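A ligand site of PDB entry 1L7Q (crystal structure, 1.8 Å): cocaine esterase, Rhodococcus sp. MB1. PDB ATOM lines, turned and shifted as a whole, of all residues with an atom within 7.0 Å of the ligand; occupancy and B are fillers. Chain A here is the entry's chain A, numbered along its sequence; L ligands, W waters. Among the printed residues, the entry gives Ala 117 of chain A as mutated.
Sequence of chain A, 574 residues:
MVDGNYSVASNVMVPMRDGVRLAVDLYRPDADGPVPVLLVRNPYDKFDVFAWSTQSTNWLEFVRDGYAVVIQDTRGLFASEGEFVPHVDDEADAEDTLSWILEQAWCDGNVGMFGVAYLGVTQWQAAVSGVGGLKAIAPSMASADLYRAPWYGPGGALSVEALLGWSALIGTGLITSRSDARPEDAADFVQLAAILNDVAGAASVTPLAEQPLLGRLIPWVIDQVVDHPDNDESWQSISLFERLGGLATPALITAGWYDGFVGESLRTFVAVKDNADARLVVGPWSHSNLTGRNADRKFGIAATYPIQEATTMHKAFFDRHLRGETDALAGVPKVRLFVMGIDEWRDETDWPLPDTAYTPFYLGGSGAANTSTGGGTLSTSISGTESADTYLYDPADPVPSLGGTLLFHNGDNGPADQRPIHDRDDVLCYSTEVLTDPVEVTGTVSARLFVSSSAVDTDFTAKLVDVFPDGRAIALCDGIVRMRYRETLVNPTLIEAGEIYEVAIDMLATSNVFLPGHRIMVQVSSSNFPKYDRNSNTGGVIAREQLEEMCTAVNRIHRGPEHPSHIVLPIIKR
OH of Tyr 44 lies within hydrogen-bond range of O1 of the ligand, 2.6 Å away. A ring nitrogen (NE2) of His 287 is in hydrogen-bond range of an oxygen (O2) of the ligand, 3.0 Å away. An oxygen (O1) of the ligand sits at hydrogen-bond distance from the backbone NH of Tyr 118 (3.2 Å).
NE1 of Trp 166 lies within hydrogen-bond range of OH of Tyr 44. OH of Tyr 118 lies within hydrogen-bond range of N of His 87, 3.2 Å away. The backbone NH (N) of Ala 117 lies close to the backbone carbonyl oxygen (O) of Met 141 (3.5 Å). The indole nitrogen of Trp 151 sits at hydrogen-bond distance from a ring nitrogen (NE2) of His 87 (3.0 Å).
Residues that only touch the ligand: Ala 117, Pro 150, Trp 151, Trp 166, Phe 261, Leu 407 and Phe 408. Ten residues have an atom within 4 Å of the ligand: Tyr 44, Ala 117, Tyr 118, Pro 150, Trp 151, Trp 166, Phe 261, His 287, Leu 407 and Phe 408. The nearest printed residue that does not touch the ligand is Val 116 (4.5 Å).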
ATOM      1  N   PRO A  43       3.115 -25.991  21.803  1.00  0.00           N
ATOM      2  CA  PRO A  43       2.909 -25.273  20.539  1.00  0.00           C
ATOM      3  C   PRO A  43       3.538 -23.870  20.570  1.00  0.00           C
ATOM      4  O   PRO A  43       3.372 -23.099  19.625  1.00  0.00           O
ATOM      5  CB  PRO A  43       1.395 -25.194  20.449  1.00  0.00           C
ATOM      6  CG  PRO A  43       1.018 -24.925  21.888  1.00  0.00           C
ATOM      7  CD  PRO A  43       1.925 -25.883  22.661  1.00  0.00           C
ATOM      8  N   TYR A  44       4.244 -23.552  21.646  1.00  0.00           N
ATOM      9  CA  TYR A  44       4.853 -22.230  21.792  1.00  0.00           C
ATOM     10  C   TYR A  44       6.381 -22.215  21.801  1.00  0.00           C
ATOM     11  O   TYR A  44       7.006 -21.405  22.492  1.00  0.00           O
ATOM     12  CB  TYR A  44       4.330 -21.588  23.091  1.00  0.00           C
ATOM     13  CG  TYR A  44       2.829 -21.711  23.266  1.00  0.00           C
ATOM     14  CD1 TYR A  44       1.946 -21.118  22.366  1.00  0.00           C
ATOM     15  CD2 TYR A  44       2.297 -22.439  24.334  1.00  0.00           C
ATOM     16  CE1 TYR A  44       0.567 -21.244  22.535  1.00  0.00           C
ATOM     17  CE2 TYR A  44       0.927 -22.576  24.502  1.00  0.00           C
ATOM     18  CZ  TYR A  44       0.057 -21.974  23.595  1.00  0.00           C
ATOM     19  OH  TYR A  44      -1.299 -22.117  23.751  1.00  0.00           O
ATOM     20  N   GLN A  55       4.752 -21.011  35.287  1.00  0.00           N
ATOM     21  CA  GLN A  55       3.356 -21.289  35.629  1.00  0.00           C
ATOM     22  C   GLN A  55       3.193 -22.782  35.879  1.00  0.00           C
ATOM     23  O   GLN A  55       2.066 -23.283  35.957  1.00  0.00           O
ATOM     24  CB  GLN A  55       2.423 -20.875  34.482  1.00  0.00           C
ATOM     25  CG  GLN A  55       2.503 -19.401  34.102  1.00  0.00           C
ATOM     26  CD  GLN A  55       3.263 -19.181  32.814  1.00  0.00           C
ATOM     27  OE1 GLN A  55       2.855 -19.624  31.740  1.00  0.00           O
ATOM     28  NE2 GLN A  55       4.397 -18.497  32.917  1.00  0.00           N
ATOM     29  N   HIS A  87      -5.567 -28.940  18.040  1.00  0.00           N
ATOM     30  CA  HIS A  87      -6.155 -30.178  18.555  1.00  0.00           C
ATOM     31  C   HIS A  87      -6.270 -31.448  17.707  1.00  0.00           C
ATOM     32  O   HIS A  87      -6.053 -32.548  18.217  1.00  0.00           O
ATOM     33  CB  HIS A  87      -7.560 -29.891  19.110  1.00  0.00           C
ATOM     34  CG  HIS A  87      -7.657 -28.606  19.873  1.00  0.00           C
ATOM     35  ND1 HIS A  87      -6.830 -28.292  20.926  1.00  0.00           N
ATOM     36  CD2 HIS A  87      -8.523 -27.558  19.748  1.00  0.00           C
ATOM     37  CE1 HIS A  87      -7.178 -27.109  21.417  1.00  0.00           C
ATOM     38  NE2 HIS A  87      -8.198 -26.656  20.724  1.00  0.00           N
ATOM     39  N   VAL A 116       0.964 -26.856  31.446  1.00  0.00           N
ATOM     40  CA  VAL A 116      -0.236 -26.059  31.639  1.00  0.00           C
ATOM     41  C   VAL A 116      -0.992 -25.665  30.366  1.00  0.00           C
ATOM     42  O   VAL A 116      -0.388 -25.438  29.313  1.00  0.00           O
ATOM     43  CB  VAL A 116       0.115 -24.773  32.423  1.00  0.00           C
ATOM     44  CG1 VAL A 116       1.191 -24.001  31.684  1.00  0.00           C
ATOM     45  CG2 VAL A 116      -1.122 -23.914  32.622  1.00  0.00           C
ATOM     46  N   ALA A 117      -2.313 -25.582  30.489  1.00  0.00           N
ATOM     47  CA  ALA A 117      -3.207 -25.192  29.397  1.00  0.00           C
ATOM     48  C   ALA A 117      -3.120 -26.098  28.167  1.00  0.00           C
ATOM     49  O   ALA A 117      -3.493 -27.265  28.233  1.00  0.00           O
ATOM     50  CB  ALA A 117      -2.929 -23.742  29.029  1.00  0.00           C
ATOM     51  N   TYR A 118      -2.646 -25.566  27.046  1.00  0.00           N
ATOM     52  CA  TYR A 118      -2.540 -26.385  25.838  1.00  0.00           C
ATOM     53  C   TYR A 118      -1.581 -27.545  26.141  1.00  0.00           C
ATOM     54  O   TYR A 118      -1.744 -28.652  25.614  1.00  0.00           O
ATOM     55  CB  TYR A 118      -2.012 -25.558  24.667  1.00  0.00           C
ATOM     56  CG  TYR A 118      -2.275 -26.170  23.303  1.00  0.00           C
ATOM     57  CD1 TYR A 118      -1.536 -27.261  22.833  1.00  0.00           C
ATOM     58  CD2 TYR A 118      -3.264 -25.643  22.463  1.00  0.00           C
ATOM     59  CE1 TYR A 118      -1.762 -27.809  21.572  1.00  0.00           C
ATOM     60  CE2 TYR A 118      -3.498 -26.189  21.191  1.00  0.00           C
ATOM     61  CZ  TYR A 118      -2.751 -27.266  20.755  1.00  0.00           C
ATOM     62  OH  TYR A 118      -2.978 -27.797  19.499  1.00  0.00           O
ATOM     63  N   LEU A 119      -0.589 -27.285  26.995  1.00  0.00           N
ATOM     64  CA  LEU A 119       0.374 -28.308  27.389  1.00  0.00           C
ATOM     65  C   LEU A 119      -0.297 -29.279  28.367  1.00  0.00           C
ATOM     66  O   LEU A 119       0.276 -30.285  28.763  1.00  0.00           O
ATOM     67  CB  LEU A 119       1.596 -27.675  28.061  1.00  0.00           C
ATOM     68  CG  LEU A 119       2.642 -27.005  27.167  1.00  0.00           C
ATOM     69  CD1 LEU A 119       2.015 -25.879  26.346  1.00  0.00           C
ATOM     70  CD2 LEU A 119       3.761 -26.448  28.051  1.00  0.00           C
ATOM     71  N   GLY A 120      -1.532 -28.945  28.752  1.00  0.00           N
ATOM     72  CA  GLY A 120      -2.303 -29.786  29.646  1.00  0.00           C
ATOM     73  C   GLY A 120      -3.315 -30.575  28.846  1.00  0.00           C
ATOM     74  O   GLY A 120      -3.522 -31.778  29.067  1.00  0.00           O
ATOM     75  N   VAL A 121      -3.962 -29.904  27.896  1.00  0.00           N
ATOM     76  CA  VAL A 121      -4.947 -30.571  27.046  1.00  0.00           C
ATOM     77  C   VAL A 121      -4.290 -31.731  26.315  1.00  0.00           C
ATOM     78  O   VAL A 121      -4.865 -32.821  26.193  1.00  0.00           O
ATOM     79  CB  VAL A 121      -5.527 -29.585  26.002  1.00  0.00           C
ATOM     80  CG1 VAL A 121      -6.399 -30.349  24.995  1.00  0.00           C
ATOM     81  CG2 VAL A 121      -6.340 -28.511  26.700  1.00  0.00           C
ATOM     82  N   MET A 141      -4.487 -26.335  34.696  1.00  0.00           N
ATOM     83  CA  MET A 141      -5.383 -25.362  34.055  1.00  0.00           C
ATOM     84  C   MET A 141      -5.721 -25.833  32.644  1.00  0.00           C
ATOM     85  O   MET A 141      -5.547 -25.109  31.658  1.00  0.00           O
ATOM     86  CB  MET A 141      -4.696 -23.985  34.052  1.00  0.00           C
ATOM     87  CG  MET A 141      -4.440 -23.479  35.480  1.00  0.00           C
ATOM     88  SD  MET A 141      -3.420 -21.995  35.584  1.00  0.00           S
ATOM     89  CE  MET A 141      -4.594 -20.780  36.188  1.00  0.00           C
ATOM     90  N   PRO A 150     -11.713 -24.171  26.223  1.00  0.00           N
ATOM     91  CA  PRO A 150     -12.048 -22.756  26.398  1.00  0.00           C
ATOM     92  C   PRO A 150     -12.818 -22.061  25.266  1.00  0.00           C
ATOM     93  O   PRO A 150     -13.072 -20.867  25.364  1.00  0.00           O
ATOM     94  CB  PRO A 150     -10.684 -22.127  26.562  1.00  0.00           C
ATOM     95  CG  PRO A 150      -9.907 -22.843  25.458  1.00  0.00           C
ATOM     96  CD  PRO A 150     -10.413 -24.294  25.512  1.00  0.00           C
ATOM     97  N   TRP A 151     -13.191 -22.782  24.221  1.00  0.00           N
ATOM     98  CA  TRP A 151     -13.841 -22.136  23.074  1.00  0.00           C
ATOM     99  C   TRP A 151     -15.312 -21.740  23.212  1.00  0.00           C
ATOM    100  O   TRP A 151     -15.702 -20.660  22.742  1.00  0.00           O
ATOM    101  CB  TRP A 151     -13.616 -23.005  21.834  1.00  0.00           C
ATOM    102  CG  TRP A 151     -12.157 -23.338  21.665  1.00  0.00           C
ATOM    103  CD1 TRP A 151     -11.629 -24.564  21.398  1.00  0.00           C
ATOM    104  CD2 TRP A 151     -11.043 -22.447  21.793  1.00  0.00           C
ATOM    105  NE1 TRP A 151     -10.256 -24.500  21.366  1.00  0.00           N
ATOM    106  CE2 TRP A 151      -9.870 -23.211  21.600  1.00  0.00           C
ATOM    107  CE3 TRP A 151     -10.919 -21.067  22.053  1.00  0.00           C
ATOM    108  CZ2 TRP A 151      -8.579 -22.646  21.671  1.00  0.00           C
ATOM    109  CZ3 TRP A 151      -9.635 -20.508  22.119  1.00  0.00           C
ATOM    110  CH2 TRP A 151      -8.486 -21.300  21.930  1.00  0.00           C
ATOM    111  N   ALA A 162     -11.638 -15.296  24.161  1.00  0.00           N
ATOM    112  CA  ALA A 162     -10.662 -16.374  24.266  1.00  0.00           C
ATOM    113  C   ALA A 162     -10.212 -16.775  22.868  1.00  0.00           C
ATOM    114  O   ALA A 162      -9.033 -16.967  22.614  1.00  0.00           O
ATOM    115  CB  ALA A 162     -11.275 -17.574  25.002  1.00  0.00           C
ATOM    116  N   LEU A 163     -11.180 -16.888  21.963  1.00  0.00           N
ATOM    117  CA  LEU A 163     -10.900 -17.296  20.588  1.00  0.00           C
ATOM    118  C   LEU A 163     -10.005 -16.316  19.837  1.00  0.00           C
ATOM    119  O   LEU A 163      -8.959 -16.696  19.298  1.00  0.00           O
ATOM    120  CB  LEU A 163     -12.198 -17.474  19.811  1.00  0.00           C
ATOM    121  CG  LEU A 163     -12.005 -17.886  18.339  1.00  0.00           C
ATOM    122  CD1 LEU A 163     -11.300 -19.238  18.288  1.00  0.00           C
ATOM    123  CD2 LEU A 163     -13.353 -17.960  17.643  1.00  0.00           C
ATOM    124  N   TRP A 166      -6.343 -15.864  21.620  1.00  0.00           N
ATOM    125  CA  TRP A 166      -5.431 -16.978  21.402  1.00  0.00           C
ATOM    126  C   TRP A 166      -5.012 -17.068  19.931  1.00  0.00           C
ATOM    127  O   TRP A 166      -3.845 -17.313  19.629  1.00  0.00           O
ATOM    128  CB  TRP A 166      -6.076 -18.304  21.805  1.00  0.00           C
ATOM    129  CG  TRP A 166      -5.102 -19.454  21.786  1.00  0.00           C
ATOM    130  CD1 TRP A 166      -4.076 -19.655  22.668  1.00  0.00           C
ATOM    131  CD2 TRP A 166      -5.047 -20.525  20.847  1.00  0.00           C
ATOM    132  NE1 TRP A 166      -3.394 -20.803  22.341  1.00  0.00           N
ATOM    133  CE2 TRP A 166      -3.963 -21.354  21.224  1.00  0.00           C
ATOM    134  CE3 TRP A 166      -5.810 -20.878  19.726  1.00  0.00           C
ATOM    135  CZ2 TRP A 166      -3.627 -22.514  20.518  1.00  0.00           C
ATOM    136  CZ3 TRP A 166      -5.476 -22.031  19.014  1.00  0.00           C
ATOM    137  CH2 TRP A 166      -4.385 -22.837  19.418  1.00  0.00           C
ATOM    138  N   LEU A 169      -2.420 -14.670  19.153  1.00  0.00           N
ATOM    139  CA  LEU A 169      -1.143 -15.099  19.722  1.00  0.00           C
ATOM    140  C   LEU A 169      -0.488 -16.158  18.840  1.00  0.00           C
ATOM    141  O   LEU A 169       0.718 -16.095  18.575  1.00  0.00           O
ATOM    142  CB  LEU A 169      -1.340 -15.652  21.131  1.00  0.00           C
ATOM    143  CG  LEU A 169      -1.481 -14.607  22.243  1.00  0.00           C
ATOM    144  CD1 LEU A 169      -1.650 -15.316  23.576  1.00  0.00           C
ATOM    145  CD2 LEU A 169      -0.249 -13.718  22.266  1.00  0.00           C
ATOM    146  N   PHE A 261     -10.225 -22.340  32.188  1.00  0.00           N
ATOM    147  CA  PHE A 261     -10.451 -23.785  32.104  1.00  0.00           C
ATOM    148  C   PHE A 261     -10.948 -24.428  33.402  1.00  0.00           C
ATOM    149  O   PHE A 261     -11.181 -25.638  33.439  1.00  0.00           O
ATOM    150  CB  PHE A 261      -9.172 -24.525  31.714  1.00  0.00           C
ATOM    151  CG  PHE A 261      -8.534 -24.042  30.434  1.00  0.00           C
ATOM    152  CD1 PHE A 261      -7.840 -22.847  30.394  1.00  0.00           C
ATOM    153  CD2 PHE A 261      -8.593 -24.829  29.281  1.00  0.00           C
ATOM    154  CE1 PHE A 261      -7.205 -22.422  29.223  1.00  0.00           C
ATOM    155  CE2 PHE A 261      -7.969 -24.422  28.106  1.00  0.00           C
ATOM    156  CZ  PHE A 261      -7.268 -23.214  28.082  1.00  0.00           C
ATOM    157  N   HIS A 287      -5.735 -17.123  34.318  1.00  0.00           N
ATOM    158  CA  HIS A 287      -4.720 -17.691  33.432  1.00  0.00           C
ATOM    159  C   HIS A 287      -3.406 -16.907  33.332  1.00  0.00           C
ATOM    160  O   HIS A 287      -2.332 -17.503  33.383  1.00  0.00           O
ATOM    161  CB  HIS A 287      -5.285 -17.873  32.027  1.00  0.00           C
ATOM    162  CG  HIS A 287      -4.704 -19.057  31.305  1.00  0.00           C
ATOM    163  ND1 HIS A 287      -5.038 -20.352  31.624  1.00  0.00           N
ATOM    164  CD2 HIS A 287      -3.799 -19.134  30.304  1.00  0.00           C
ATOM    165  CE1 HIS A 287      -4.361 -21.181  30.849  1.00  0.00           C
ATOM    166  NE2 HIS A 287      -3.601 -20.458  30.039  1.00  0.00           N
ATOM    167  N   LEU A 407      -9.760 -14.633  29.642  1.00  0.00           N
ATOM    168  CA  LEU A 407      -8.432 -15.156  29.334  1.00  0.00           C
ATOM    169  C   LEU A 407      -7.478 -14.132  28.738  1.00  0.00           C
ATOM    170  O   LEU A 407      -6.350 -13.983  29.213  1.00  0.00           O
ATOM    171  CB  LEU A 407      -8.553 -16.356  28.395  1.00  0.00           C
ATOM    172  CG  LEU A 407      -9.078 -17.647  29.023  1.00  0.00           C
ATOM    173  CD1 LEU A 407      -9.360 -18.683  27.928  1.00  0.00           C
ATOM    174  CD2 LEU A 407      -8.059 -18.179  30.011  1.00  0.00           C
ATOM    175  N   PHE A 408      -7.925 -13.410  27.713  1.00  0.00           N
ATOM    176  CA  PHE A 408      -7.072 -12.428  27.042  1.00  0.00           C
ATOM    177  C   PHE A 408      -7.491 -10.979  27.217  1.00  0.00           C
ATOM    178  O   PHE A 408      -6.645 -10.090  27.318  1.00  0.00           O
ATOM    179  CB  PHE A 408      -6.967 -12.792  25.559  1.00  0.00           C
ATOM    180  CG  PHE A 408      -6.307 -14.112  25.330  1.00  0.00           C
ATOM    181  CD1 PHE A 408      -4.939 -14.254  25.514  1.00  0.00           C
ATOM    182  CD2 PHE A 408      -7.060 -15.229  24.976  1.00  0.00           C
ATOM    183  CE1 PHE A 408      -4.331 -15.501  25.361  1.00  0.00           C
ATOM    184  CE2 PHE A 408      -6.461 -16.464  24.824  1.00  0.00           C
ATOM    185  CZ  PHE A 408      -5.092 -16.614  25.014  1.00  0.00           C
HETATM  186  C1  LIG L   1      -2.675 -21.629  26.581  1.00  0.00           C
HETATM  187  O1  LIG L   1      -2.005 -22.579  26.197  1.00  0.00           O
HETATM  188  O2  LIG L   1      -2.198 -20.847  27.409  1.00  0.00           O
HETATM  189  C2  LIG L   1      -4.098 -21.362  26.111  1.00  0.00           C
HETATM  190  C3  LIG L   1      -4.717 -20.223  26.689  1.00  0.00           C
HETATM  191  C4  LIG L   1      -6.126 -19.955  26.217  1.00  0.00           C
HETATM  192  C5  LIG L   1      -6.787 -20.806  25.253  1.00  0.00           C
HETATM  193  C6  LIG L   1      -6.151 -21.958  24.686  1.00  0.00           C
HETATM  194  C7  LIG L   1      -4.811 -22.209  25.135  1.00  0.00           C
HETATM  195  O   HOH W   1      -1.634 -18.698  25.842  1.00  0.00           O
HETATM  196  O   HOH W   2       0.405 -21.830  28.636  1.00  0.00           O
